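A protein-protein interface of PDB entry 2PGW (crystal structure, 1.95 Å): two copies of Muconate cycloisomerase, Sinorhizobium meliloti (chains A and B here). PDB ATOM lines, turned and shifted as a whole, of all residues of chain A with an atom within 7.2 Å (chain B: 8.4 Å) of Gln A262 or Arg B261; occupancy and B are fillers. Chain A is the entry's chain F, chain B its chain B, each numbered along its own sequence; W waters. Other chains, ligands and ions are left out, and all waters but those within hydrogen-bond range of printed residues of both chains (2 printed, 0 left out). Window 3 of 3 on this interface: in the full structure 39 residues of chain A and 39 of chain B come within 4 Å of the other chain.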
ATOM      1  N   SER A 229     -30.382  13.670 -35.344  1.00  0.00           N
ATOM      2  CA  SER A 229     -30.176  14.247 -34.013  1.00  0.00           C
ATOM      3  C   SER A 229     -30.364  13.265 -32.869  1.00  0.00           C
ATOM      4  O   SER A 229     -31.498  12.944 -32.496  1.00  0.00           O
ATOM      5  CB  SER A 229     -31.104  15.451 -33.791  1.00  0.00           C
ATOM      6  OG  SER A 229     -30.992  15.969 -32.465  1.00  0.00           O
ATOM      7  N   ILE A 230     -29.250  12.804 -32.311  1.00  0.00           N
ATOM      8  CA  ILE A 230     -29.289  11.898 -31.174  1.00  0.00           C
ATOM      9  C   ILE A 230     -29.920  12.650 -29.996  1.00  0.00           C
ATOM     10  O   ILE A 230     -30.742  12.094 -29.280  1.00  0.00           O
ATOM     11  CB  ILE A 230     -27.872  11.386 -30.799  1.00  0.00           C
ATOM     12  CG1 ILE A 230     -27.274  10.595 -31.971  1.00  0.00           C
ATOM     13  CG2 ILE A 230     -27.939  10.511 -29.554  1.00  0.00           C
ATOM     14  CD1 ILE A 230     -28.080   9.385 -32.377  1.00  0.00           C
ATOM     15  N   PRO A 231     -29.538  13.929 -29.782  1.00  0.00           N
ATOM     16  CA  PRO A 231     -30.106  14.716 -28.679  1.00  0.00           C
ATOM     17  C   PRO A 231     -31.625  14.852 -28.743  1.00  0.00           C
ATOM     18  O   PRO A 231     -32.307  14.788 -27.718  1.00  0.00           O
ATOM     19  CB  PRO A 231     -29.400  16.056 -28.823  1.00  0.00           C
ATOM     20  CG  PRO A 231     -28.043  15.638 -29.229  1.00  0.00           C
ATOM     21  CD  PRO A 231     -28.338  14.604 -30.310  1.00  0.00           C
ATOM     22  N   ALA A 232     -32.153  15.046 -29.947  1.00  0.00           N
ATOM     23  CA  ALA A 232     -33.596  15.179 -30.121  1.00  0.00           C
ATOM     24  C   ALA A 232     -34.310  13.893 -29.689  1.00  0.00           C
ATOM     25  O   ALA A 232     -35.376  13.945 -29.080  1.00  0.00           O
ATOM     26  CB  ALA A 232     -33.924  15.501 -31.577  1.00  0.00           C
ATOM     27  N   ALA A 234     -33.161  11.610 -27.455  1.00  0.00           N
ATOM     28  CA  ALA A 234     -33.085  11.481 -26.001  1.00  0.00           C
ATOM     29  C   ALA A 234     -34.143  12.397 -25.374  1.00  0.00           C
ATOM     30  O   ALA A 234     -34.810  12.027 -24.410  1.00  0.00           O
ATOM     31  CB  ALA A 234     -31.692  11.863 -25.502  1.00  0.00           C
ATOM     32  N   ARG A 237     -37.422  10.679 -25.640  1.00  0.00           N
ATOM     33  CA  ARG A 237     -37.445   9.497 -24.768  1.00  0.00           C
ATOM     34  C   ARG A 237     -37.683   9.830 -23.300  1.00  0.00           C
ATOM     35  O   ARG A 237     -38.496   9.198 -22.625  1.00  0.00           O
ATOM     36  CB  ARG A 237     -36.141   8.705 -24.876  1.00  0.00           C
ATOM     37  CG  ARG A 237     -36.132   7.453 -23.995  1.00  0.00           C
ATOM     38  CD  ARG A 237     -34.741   6.847 -23.906  1.00  0.00           C
ATOM     39  NE  ARG A 237     -33.849   7.590 -23.003  1.00  0.00           N
ATOM     40  CZ  ARG A 237     -34.011   7.676 -21.688  1.00  0.00           C
ATOM     41  NH1 ARG A 237     -35.035   7.080 -21.103  1.00  0.00           N
ATOM     42  NH2 ARG A 237     -33.121   8.347 -20.947  1.00  0.00           N
ATOM     43  N   GLU A 238     -36.955  10.825 -22.810  1.00  0.00           N
ATOM     44  CA  GLU A 238     -37.059  11.246 -21.427  1.00  0.00           C
ATOM     45  C   GLU A 238     -38.434  11.805 -21.077  1.00  0.00           C
ATOM     46  O   GLU A 238     -38.812  11.830 -19.911  1.00  0.00           O
ATOM     47  CB  GLU A 238     -35.985  12.296 -21.129  1.00  0.00           C
ATOM     48  CG  GLU A 238     -34.571  11.735 -21.028  1.00  0.00           C
ATOM     49  CD  GLU A 238     -33.518  12.829 -20.974  1.00  0.00           C
ATOM     50  OE1 GLU A 238     -33.725  13.819 -20.237  1.00  0.00           O
ATOM     51  OE2 GLU A 238     -32.480  12.702 -21.662  1.00  0.00           O
ATOM     52  N   ASP A 255     -22.002   5.876 -33.774  1.00  0.00           N
ATOM     53  CA  ASP A 255     -23.382   6.292 -33.542  1.00  0.00           C
ATOM     54  C   ASP A 255     -23.903   5.495 -32.337  1.00  0.00           C
ATOM     55  O   ASP A 255     -24.529   6.049 -31.422  1.00  0.00           O
ATOM     56  CB  ASP A 255     -24.277   5.994 -34.751  1.00  0.00           C
ATOM     57  CG  ASP A 255     -23.981   6.879 -35.937  1.00  0.00           C
ATOM     58  OD1 ASP A 255     -23.482   7.998 -35.740  1.00  0.00           O
ATOM     59  OD2 ASP A 255     -24.268   6.453 -37.070  1.00  0.00           O
ATOM     60  N   VAL A 256     -23.641   4.190 -32.349  1.00  0.00           N
ATOM     61  CA  VAL A 256     -24.072   3.316 -31.261  1.00  0.00           C
ATOM     62  C   VAL A 256     -23.516   3.801 -29.913  1.00  0.00           C
ATOM     63  O   VAL A 256     -24.244   3.889 -28.920  1.00  0.00           O
ATOM     64  CB  VAL A 256     -23.631   1.855 -31.506  1.00  0.00           C
ATOM     65  CG1 VAL A 256     -23.897   1.006 -30.258  1.00  0.00           C
ATOM     66  CG2 VAL A 256     -24.384   1.282 -32.707  1.00  0.00           C
ATOM     67  N   TYR A 257     -22.227   4.123 -29.884  1.00  0.00           N
ATOM     68  CA  TYR A 257     -21.596   4.608 -28.660  1.00  0.00           C
ATOM     69  C   TYR A 257     -22.241   5.923 -28.178  1.00  0.00           C
ATOM     70  O   TYR A 257     -22.438   6.122 -26.980  1.00  0.00           O
ATOM     71  CB  TYR A 257     -20.096   4.817 -28.885  1.00  0.00           C
ATOM     72  CG  TYR A 257     -19.356   5.291 -27.653  1.00  0.00           C
ATOM     73  CD1 TYR A 257     -19.254   4.481 -26.522  1.00  0.00           C
ATOM     74  CD2 TYR A 257     -18.772   6.557 -27.612  1.00  0.00           C
ATOM     75  CE1 TYR A 257     -18.584   4.928 -25.367  1.00  0.00           C
ATOM     76  CE2 TYR A 257     -18.099   7.017 -26.473  1.00  0.00           C
ATOM     77  CZ  TYR A 257     -18.010   6.198 -25.353  1.00  0.00           C
ATOM     78  OH  TYR A 257     -17.341   6.646 -24.233  1.00  0.00           O
ATOM     79  N   GLU A 258     -22.567   6.816 -29.116  1.00  0.00           N
ATOM     80  CA  GLU A 258     -23.187   8.090 -28.751  1.00  0.00           C
ATOM     81  C   GLU A 258     -24.570   7.884 -28.151  1.00  0.00           C
ATOM     82  O   GLU A 258     -24.907   8.493 -27.141  1.00  0.00           O
ATOM     83  CB  GLU A 258     -23.289   9.007 -29.966  1.00  0.00           C
ATOM     84  CG  GLU A 258     -21.976   9.663 -30.331  1.00  0.00           C
ATOM     85  CD  GLU A 258     -21.437  10.521 -29.200  1.00  0.00           C
ATOM     86  OE1 GLU A 258     -22.117  11.495 -28.816  1.00  0.00           O
ATOM     87  OE2 GLU A 258     -20.339  10.211 -28.691  1.00  0.00           O
ATOM     88  N   ILE A 259     -25.373   7.037 -28.785  1.00  0.00           N
ATOM     89  CA  ILE A 259     -26.706   6.753 -28.264  1.00  0.00           C
ATOM     90  C   ILE A 259     -26.575   6.172 -26.852  1.00  0.00           C
ATOM     91  O   ILE A 259     -27.311   6.560 -25.949  1.00  0.00           O
ATOM     92  CB  ILE A 259     -27.441   5.768 -29.180  1.00  0.00           C
ATOM     93  CG1 ILE A 259     -27.681   6.437 -30.534  1.00  0.00           C
ATOM     94  CG2 ILE A 259     -28.741   5.312 -28.532  1.00  0.00           C
ATOM     95  CD1 ILE A 259     -28.145   5.485 -31.614  1.00  0.00           C
ATOM     96  N   CYS A 260     -25.628   5.249 -26.665  1.00  0.00           N
ATOM     97  CA  CYS A 260     -25.397   4.638 -25.350  1.00  0.00           C
ATOM     98  C   CYS A 260     -24.972   5.687 -24.316  1.00  0.00           C
ATOM     99  O   CYS A 260     -25.570   5.827 -23.241  1.00  0.00           O
ATOM    100  CB  CYS A 260     -24.298   3.570 -25.439  1.00  0.00           C
ATOM    101  SG  CYS A 260     -24.801   2.051 -26.265  1.00  0.00           S
ATOM    102  N   ARG A 261     -23.915   6.403 -24.661  1.00  0.00           N
ATOM    103  CA  ARG A 261     -23.327   7.447 -23.824  1.00  0.00           C
ATOM    104  C   ARG A 261     -24.365   8.475 -23.366  1.00  0.00           C
ATOM    105  O   ARG A 261     -24.358   8.919 -22.212  1.00  0.00           O
ATOM    106  CB  ARG A 261     -22.216   8.124 -24.642  1.00  0.00           C
ATOM    107  CG  ARG A 261     -21.457   9.227 -23.971  1.00  0.00           C
ATOM    108  CD  ARG A 261     -20.258   9.601 -24.837  1.00  0.00           C
ATOM    109  NE  ARG A 261     -20.558  10.580 -25.890  1.00  0.00           N
ATOM    110  CZ  ARG A 261     -20.729  11.883 -25.673  1.00  0.00           C
ATOM    111  NH1 ARG A 261     -20.640  12.369 -24.440  1.00  0.00           N
ATOM    112  NH2 ARG A 261     -20.953  12.712 -26.683  1.00  0.00           N
ATOM    113  N   GLN A 262     -25.265   8.839 -24.272  1.00  0.00           N
ATOM    114  CA  GLN A 262     -26.300   9.814 -23.979  1.00  0.00           C
ATOM    115  C   GLN A 262     -27.606   9.182 -23.496  1.00  0.00           C
ATOM    116  O   GLN A 262     -28.566   9.901 -23.235  1.00  0.00           O
ATOM    117  CB  GLN A 262     -26.587  10.652 -25.231  1.00  0.00           C
ATOM    118  CG  GLN A 262     -25.408  11.486 -25.723  1.00  0.00           C
ATOM    119  CD  GLN A 262     -25.674  12.138 -27.069  1.00  0.00           C
ATOM    120  OE1 GLN A 262     -26.678  12.817 -27.247  1.00  0.00           O
ATOM    121  NE2 GLN A 262     -24.771  11.933 -28.016  1.00  0.00           N
ATOM    122  N   ARG A 263     -27.635   7.856 -23.368  1.00  0.00           N
ATOM    123  CA  ARG A 263     -28.847   7.142 -22.955  1.00  0.00           C
ATOM    124  C   ARG A 263     -30.012   7.660 -23.817  1.00  0.00           C
ATOM    125  O   ARG A 263     -31.101   7.942 -23.310  1.00  0.00           O
ATOM    126  CB  ARG A 263     -29.168   7.386 -21.463  1.00  0.00           C
ATOM    127  CG  ARG A 263     -28.009   7.193 -20.460  1.00  0.00           C
ATOM    128  CD  ARG A 263     -27.341   5.818 -20.534  1.00  0.00           C
ATOM    129  NE  ARG A 263     -28.262   4.687 -20.376  1.00  0.00           N
ATOM    130  CZ  ARG A 263     -27.874   3.412 -20.391  1.00  0.00           C
ATOM    131  NH1 ARG A 263     -26.592   3.110 -20.544  1.00  0.00           N
ATOM    132  NH2 ARG A 263     -28.761   2.433 -20.275  1.00  0.00           N
ATOM    133  N   ALA A 264     -29.774   7.771 -25.122  1.00  0.00           N
ATOM    134  CA  ALA A 264     -30.770   8.296 -26.049  1.00  0.00           C
ATOM    135  C   ALA A 264     -31.858   7.321 -26.490  1.00  0.00           C
ATOM    136  O   ALA A 264     -32.839   7.733 -27.108  1.00  0.00           O
ATOM    137  CB  ALA A 264     -30.072   8.871 -27.274  1.00  0.00           C
ATOM    138  N   ALA A 265     -31.689   6.043 -26.182  1.00  0.00           N
ATOM    139  CA  ALA A 265     -32.670   5.039 -26.569  1.00  0.00           C
ATOM    140  C   ALA A 265     -32.743   3.910 -25.550  1.00  0.00           C
ATOM    141  O   ALA A 265     -31.804   3.690 -24.775  1.00  0.00           O
ATOM    142  CB  ALA A 265     -32.327   4.481 -27.955  1.00  0.00           C
ATOM    143  N   ILE B 230     -16.063  12.752 -31.794  1.00  0.00           N
ATOM    144  CA  ILE B 230     -16.045  14.148 -31.393  1.00  0.00           C
ATOM    145  C   ILE B 230     -15.606  14.217 -29.916  1.00  0.00           C
ATOM    146  O   ILE B 230     -14.871  15.125 -29.532  1.00  0.00           O
ATOM    147  CB  ILE B 230     -17.434  14.816 -31.623  1.00  0.00           C
ATOM    148  CG1 ILE B 230     -17.689  14.927 -33.132  1.00  0.00           C
ATOM    149  CG2 ILE B 230     -17.480  16.215 -31.003  1.00  0.00           C
ATOM    150  CD1 ILE B 230     -19.054  15.465 -33.487  1.00  0.00           C
ATOM    151  N   PRO B 231     -16.050  13.262 -29.068  1.00  0.00           N
ATOM    152  CA  PRO B 231     -15.621  13.308 -27.661  1.00  0.00           C
ATOM    153  C   PRO B 231     -14.104  13.190 -27.519  1.00  0.00           C
ATOM    154  O   PRO B 231     -13.497  13.878 -26.705  1.00  0.00           O
ATOM    155  CB  PRO B 231     -16.343  12.122 -27.046  1.00  0.00           C
ATOM    156  CG  PRO B 231     -17.657  12.150 -27.773  1.00  0.00           C
ATOM    157  CD  PRO B 231     -17.209  12.357 -29.217  1.00  0.00           C
ATOM    158  N   ALA B 234     -12.548  16.531 -28.209  1.00  0.00           N
ATOM    159  CA  ALA B 234     -12.736  17.470 -27.102  1.00  0.00           C
ATOM    160  C   ALA B 234     -11.783  17.083 -25.976  1.00  0.00           C
ATOM    161  O   ALA B 234     -11.235  17.947 -25.296  1.00  0.00           O
ATOM    162  CB  ALA B 234     -14.196  17.433 -26.602  1.00  0.00           C
ATOM    163  N   TYR B 254     -25.276  18.637 -38.619  1.00  0.00           N
ATOM    164  CA  TYR B 254     -25.386  18.015 -37.314  1.00  0.00           C
ATOM    165  C   TYR B 254     -24.025  17.815 -36.651  1.00  0.00           C
ATOM    166  O   TYR B 254     -23.904  17.974 -35.438  1.00  0.00           O
ATOM    167  CB  TYR B 254     -26.164  16.706 -37.453  1.00  0.00           C
ATOM    168  CG  TYR B 254     -27.557  16.947 -37.997  1.00  0.00           C
ATOM    169  CD1 TYR B 254     -28.601  17.303 -37.148  1.00  0.00           C
ATOM    170  CD2 TYR B 254     -27.814  16.894 -39.369  1.00  0.00           C
ATOM    171  CE1 TYR B 254     -29.864  17.608 -37.645  1.00  0.00           C
ATOM    172  CE2 TYR B 254     -29.073  17.200 -39.881  1.00  0.00           C
ATOM    173  CZ  TYR B 254     -30.091  17.558 -39.010  1.00  0.00           C
ATOM    174  OH  TYR B 254     -31.340  17.872 -39.493  1.00  0.00           O
ATOM    175  N   ASP B 255     -23.001  17.480 -37.436  1.00  0.00           N
ATOM    176  CA  ASP B 255     -21.668  17.306 -36.871  1.00  0.00           C
ATOM    177  C   ASP B 255     -21.221  18.654 -36.299  1.00  0.00           C
ATOM    178  O   ASP B 255     -20.672  18.728 -35.198  1.00  0.00           O
ATOM    179  CB  ASP B 255     -20.652  16.873 -37.936  1.00  0.00           C
ATOM    180  CG  ASP B 255     -20.962  15.511 -38.545  1.00  0.00           C
ATOM    181  OD1 ASP B 255     -21.542  14.655 -37.843  1.00  0.00           O
ATOM    182  OD2 ASP B 255     -20.601  15.295 -39.723  1.00  0.00           O
ATOM    183  N   VAL B 256     -21.442  19.712 -37.080  1.00  0.00           N
ATOM    184  CA  VAL B 256     -21.072  21.063 -36.667  1.00  0.00           C
ATOM    185  C   VAL B 256     -21.741  21.433 -35.333  1.00  0.00           C
ATOM    186  O   VAL B 256     -21.075  21.926 -34.420  1.00  0.00           O
ATOM    187  CB  VAL B 256     -21.451  22.097 -37.762  1.00  0.00           C
ATOM    188  CG1 VAL B 256     -21.125  23.519 -37.293  1.00  0.00           C
ATOM    189  CG2 VAL B 256     -20.682  21.779 -39.048  1.00  0.00           C
ATOM    190  N   TYR B 257     -23.044  21.182 -35.224  1.00  0.00           N
ATOM    191  CA  TYR B 257     -23.790  21.481 -34.004  1.00  0.00           C
ATOM    192  C   TYR B 257     -23.221  20.682 -32.828  1.00  0.00           C
ATOM    193  O   TYR B 257     -23.088  21.209 -31.722  1.00  0.00           O
ATOM    194  CB  TYR B 257     -25.280  21.132 -34.176  1.00  0.00           C
ATOM    195  CG  TYR B 257     -26.126  21.403 -32.946  1.00  0.00           C
ATOM    196  CD1 TYR B 257     -26.371  22.710 -32.518  1.00  0.00           C
ATOM    197  CD2 TYR B 257     -26.671  20.352 -32.196  1.00  0.00           C
ATOM    198  CE1 TYR B 257     -27.138  22.967 -31.375  1.00  0.00           C
ATOM    199  CE2 TYR B 257     -27.437  20.604 -31.044  1.00  0.00           C
ATOM    200  CZ  TYR B 257     -27.663  21.915 -30.648  1.00  0.00           C
ATOM    201  OH  TYR B 257     -28.415  22.177 -29.528  1.00  0.00           O
ATOM    202  N   GLU B 258     -22.887  19.419 -33.077  1.00  0.00           N
ATOM    203  CA  GLU B 258     -22.335  18.565 -32.032  1.00  0.00           C
ATOM    204  C   GLU B 258     -20.988  19.082 -31.548  1.00  0.00           C
ATOM    205  O   GLU B 258     -20.716  19.105 -30.346  1.00  0.00           O
ATOM    206  CB  GLU B 258     -22.191  17.122 -32.527  1.00  0.00           C
ATOM    207  CG  GLU B 258     -23.500  16.354 -32.528  1.00  0.00           C
ATOM    208  CD  GLU B 258     -24.158  16.359 -31.169  1.00  0.00           C
ATOM    209  OE1 GLU B 258     -23.537  15.857 -30.207  1.00  0.00           O
ATOM    210  OE2 GLU B 258     -25.289  16.873 -31.062  1.00  0.00           O
ATOM    211  N   ILE B 259     -20.147  19.497 -32.485  1.00  0.00           N
ATOM    212  CA  ILE B 259     -18.840  20.016 -32.132  1.00  0.00           C
ATOM    213  C   ILE B 259     -19.019  21.281 -31.298  1.00  0.00           C
ATOM    214  O   ILE B 259     -18.322  21.459 -30.310  1.00  0.00           O
ATOM    215  CB  ILE B 259     -17.993  20.297 -33.394  1.00  0.00           C
ATOM    216  CG1 ILE B 259     -17.629  18.963 -34.060  1.00  0.00           C
ATOM    217  CG2 ILE B 259     -16.748  21.091 -33.032  1.00  0.00           C
ATOM    218  CD1 ILE B 259     -17.043  19.101 -35.456  1.00  0.00           C
ATOM    219  N   CYS B 260     -19.980  22.123 -31.681  1.00  0.00           N
ATOM    220  CA  CYS B 260     -20.268  23.370 -30.959  1.00  0.00           C
ATOM    221  C   CYS B 260     -20.810  23.074 -29.562  1.00  0.00           C
ATOM    222  O   CYS B 260     -20.311  23.586 -28.558  1.00  0.00           O
ATOM    223  CB  CYS B 260     -21.301  24.214 -31.722  1.00  0.00           C
ATOM    224  SG  CYS B 260     -20.696  24.918 -33.281  1.00  0.00           S
ATOM    225  N   ARG B 261     -21.838  22.237 -29.526  1.00  0.00           N
ATOM    226  CA  ARG B 261     -22.499  21.831 -28.293  1.00  0.00           C
ATOM    227  C   ARG B 261     -21.520  21.243 -27.282  1.00  0.00           C
ATOM    228  O   ARG B 261     -21.645  21.470 -26.078  1.00  0.00           O
ATOM    229  CB  ARG B 261     -23.570  20.787 -28.635  1.00  0.00           C
ATOM    230  CG  ARG B 261     -24.472  20.379 -27.499  1.00  0.00           C
ATOM    231  CD  ARG B 261     -25.574  19.453 -28.005  1.00  0.00           C
ATOM    232  NE  ARG B 261     -25.112  18.082 -28.214  1.00  0.00           N
ATOM    233  CZ  ARG B 261     -24.840  17.231 -27.228  1.00  0.00           C
ATOM    234  NH1 ARG B 261     -24.981  17.601 -25.961  1.00  0.00           N
ATOM    235  NH2 ARG B 261     -24.441  15.997 -27.506  1.00  0.00           N
ATOM    236  N   GLN B 262     -20.551  20.479 -27.775  1.00  0.00           N
ATOM    237  CA  GLN B 262     -19.574  19.831 -26.908  1.00  0.00           C
ATOM    238  C   GLN B 262     -18.292  20.637 -26.742  1.00  0.00           C
ATOM    239  O   GLN B 262     -17.380  20.193 -26.047  1.00  0.00           O
ATOM    240  CB  GLN B 262     -19.239  18.438 -27.452  1.00  0.00           C
ATOM    241  CG  GLN B 262     -20.432  17.494 -27.525  1.00  0.00           C
ATOM    242  CD  GLN B 262     -20.096  16.150 -28.156  1.00  0.00           C
ATOM    243  OE1 GLN B 262     -19.076  15.535 -27.836  1.00  0.00           O
ATOM    244  NE2 GLN B 262     -20.962  15.682 -29.044  1.00  0.00           N
ATOM    245  N   ARG B 263     -18.220  21.810 -27.373  1.00  0.00           N
ATOM    246  CA  ARG B 263     -17.019  22.640 -27.282  1.00  0.00           C
ATOM    247  C   ARG B 263     -15.829  21.774 -27.668  1.00  0.00           C
ATOM    248  O   ARG B 263     -14.771  21.843 -27.050  1.00  0.00           O
ATOM    249  CB  ARG B 263     -16.836  23.154 -25.846  1.00  0.00           C
ATOM    250  CG  ARG B 263     -17.775  24.275 -25.486  1.00  0.00           C
ATOM    251  CD  ARG B 263     -17.425  25.496 -26.316  1.00  0.00           C
ATOM    252  NE  ARG B 263     -18.599  26.285 -26.604  1.00  0.00           N
ATOM    253  CZ  ARG B 263     -18.615  27.346 -27.401  1.00  0.00           C
ATOM    254  NH1 ARG B 263     -17.503  27.756 -27.998  1.00  0.00           N
ATOM    255  NH2 ARG B 263     -19.753  27.983 -27.601  1.00  0.00           N
ATOM    256  N   ALA B 264     -16.007  20.973 -28.713  1.00  0.00           N
ATOM    257  CA  ALA B 264     -14.967  20.054 -29.153  1.00  0.00           C
ATOM    258  C   ALA B 264     -13.806  20.637 -29.960  1.00  0.00           C
ATOM    259  O   ALA B 264     -12.772  19.987 -30.108  1.00  0.00           O
ATOM    260  CB  ALA B 264     -15.607  18.901 -29.920  1.00  0.00           C
ATOM    261  N   ALA B 265     -13.967  21.850 -30.477  1.00  0.00           N
ATOM    262  CA  ALA B 265     -12.899  22.466 -31.267  1.00  0.00           C
ATOM    263  C   ALA B 265     -12.891  23.973 -31.063  1.00  0.00           C
ATOM    264  O   ALA B 265     -13.874  24.544 -30.597  1.00  0.00           O
ATOM    265  CB  ALA B 265     -13.082  22.124 -32.760  1.00  0.00           C
ATOM    266  N   ILE B 268     -13.868  25.671 -36.729  1.00  0.00           N
ATOM    267  CA  ILE B 268     -14.295  24.561 -37.571  1.00  0.00           C
ATOM    268  C   ILE B 268     -13.864  24.760 -39.028  1.00  0.00           C
ATOM    269  O   ILE B 268     -14.168  25.783 -39.640  1.00  0.00           O
ATOM    270  CB  ILE B 268     -15.826  24.389 -37.486  1.00  0.00           C
ATOM    271  CG1 ILE B 268     -16.218  24.062 -36.036  1.00  0.00           C
ATOM    272  CG2 ILE B 268     -16.292  23.299 -38.430  1.00  0.00           C
ATOM    273  CD1 ILE B 268     -17.708  24.067 -35.796  1.00  0.00           C
ATOM    274  N   VAL B 287     -24.524  28.258 -37.418  1.00  0.00           N
ATOM    275  CA  VAL B 287     -24.472  27.467 -36.184  1.00  0.00           C
ATOM    276  C   VAL B 287     -23.175  27.783 -35.442  1.00  0.00           C
ATOM    277  O   VAL B 287     -23.193  27.997 -34.228  1.00  0.00           O
ATOM    278  CB  VAL B 287     -24.570  25.947 -36.484  1.00  0.00           C
ATOM    279  CG1 VAL B 287     -24.376  25.148 -35.204  1.00  0.00           C
ATOM    280  CG2 VAL B 287     -25.932  25.626 -37.080  1.00  0.00           C
ATOM    281  N   ALA B 291     -22.513  29.799 -31.745  1.00  0.00           N
ATOM    282  CA  ALA B 291     -21.695  29.162 -30.715  1.00  0.00           C
ATOM    283  C   ALA B 291     -20.392  29.932 -30.442  1.00  0.00           C
ATOM    284  O   ALA B 291     -19.531  29.461 -29.701  1.00  0.00           O
ATOM    285  CB  ALA B 291     -21.376  27.711 -31.133  1.00  0.00           C
ATOM    286  N   LEU B 293     -18.063  30.578 -32.621  1.00  0.00           N
ATOM    287  CA  LEU B 293     -16.953  29.989 -33.358  1.00  0.00           C
ATOM    288  C   LEU B 293     -16.867  30.467 -34.803  1.00  0.00           C
ATOM    289  O   LEU B 293     -17.860  30.899 -35.391  1.00  0.00           O
ATOM    290  CB  LEU B 293     -17.064  28.465 -33.329  1.00  0.00           C
ATOM    291  CG  LEU B 293     -16.918  27.808 -31.954  1.00  0.00           C
ATOM    292  CD1 LEU B 293     -17.156  26.306 -32.101  1.00  0.00           C
ATOM    293  CD2 LEU B 293     -15.533  28.089 -31.377  1.00  0.00           C
HETATM  294  O   HOH W   1     -20.961  13.121 -31.067  1.00  0.00           O
HETATM  295  O   HOH W   2     -24.638  13.109 -30.847  1.00  0.00           O
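Pro A231 touches Glu B258, and with the chains exchanged Glu A258 touches Pro B231. Pro A231 touches Arg B261, and with the chains exchanged Arg A261 touches Pro B231. Arg A261 touches Gln B262, and with the chains exchanged Gln A262 touches Arg B261. 14 positions are printed for both chains. Of the 6 pairs that touch across the chains among the printed residues, 6 have their exchanged pair printed and touching as well.
Ile A230 touches none of the printed residues of chain B. Printed residues of chain B within 4 Å of Pro A231: Glu B258 and Arg B261. Ala A232 touches none of the printed residues of chain B. Printed residues of chain B within 4 Å of Glu A258: Pro B231. Of the printed residues of chain B, Arg A261 touches Pro B231 and Gln B262. Gln A262 touches just one residue of chain B: Arg B261 (3.9 Å). Of the printed residues of chain A, Glu B258 touches Pro A231 (3.5 Å). Of the printed residues of chain A, Gln B262 touches Arg A261 (3.6 Å). The nearest residue of chain B that does not touch Gln A262 is Glu B258 (4.7 Å). The nearest residue of chain A that does not touch Arg B261 is Arg A261 (4.9 Å). The nearest printed residue of chain A that does not touch Pro B231 is Tyr A257 (5.3 Å).
NH2 of Arg B261 lies within salt-bridge range of OE1 of Glu B258, at 2.9 Å. The side-chain amide nitrogen of Gln B262 lies within hydrogen-bond range of the side-chain carboxylate of Glu B258 (2.8 Å). OE1 of Glu A258 lies within salt-bridge range of NH2 of Arg A261, 2.7 Å away. The side-chain carboxylate (OE1) of Glu A258 sits at hydrogen-bond distance from the side-chain amide nitrogen (NE2) of Gln A262 (2.8 Å).
Among the printed residues, 6 pairs touch across the chains. Among the printed residues, no Asp or Glu carboxylate lies within 4 Å of a Lys or Arg side-chain nitrogen of the other chain.
Water W1 bridges OE1 of Glu A258 and NE2 of Gln B262. Water W2 bridges OE1 of Glu B258 (3.0 Å) and NE2 of Gln A262 (3.1 Å).
Glu B258 touches Pro A231 (OE2 to CG, 3.5 Å). Arg B261 touches Pro A231. Glu A258 touches Pro B231 (OE2 to CG, 3.4 Å). Arg A261 touches Pro B231 (NH2 to CG, 3.5 Å). Gln B262 touches Arg A261 (OE1 to NH2, 3.6 Å). Gln A262 touches Arg B261 (OE1 to NH2, 3.9 Å).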
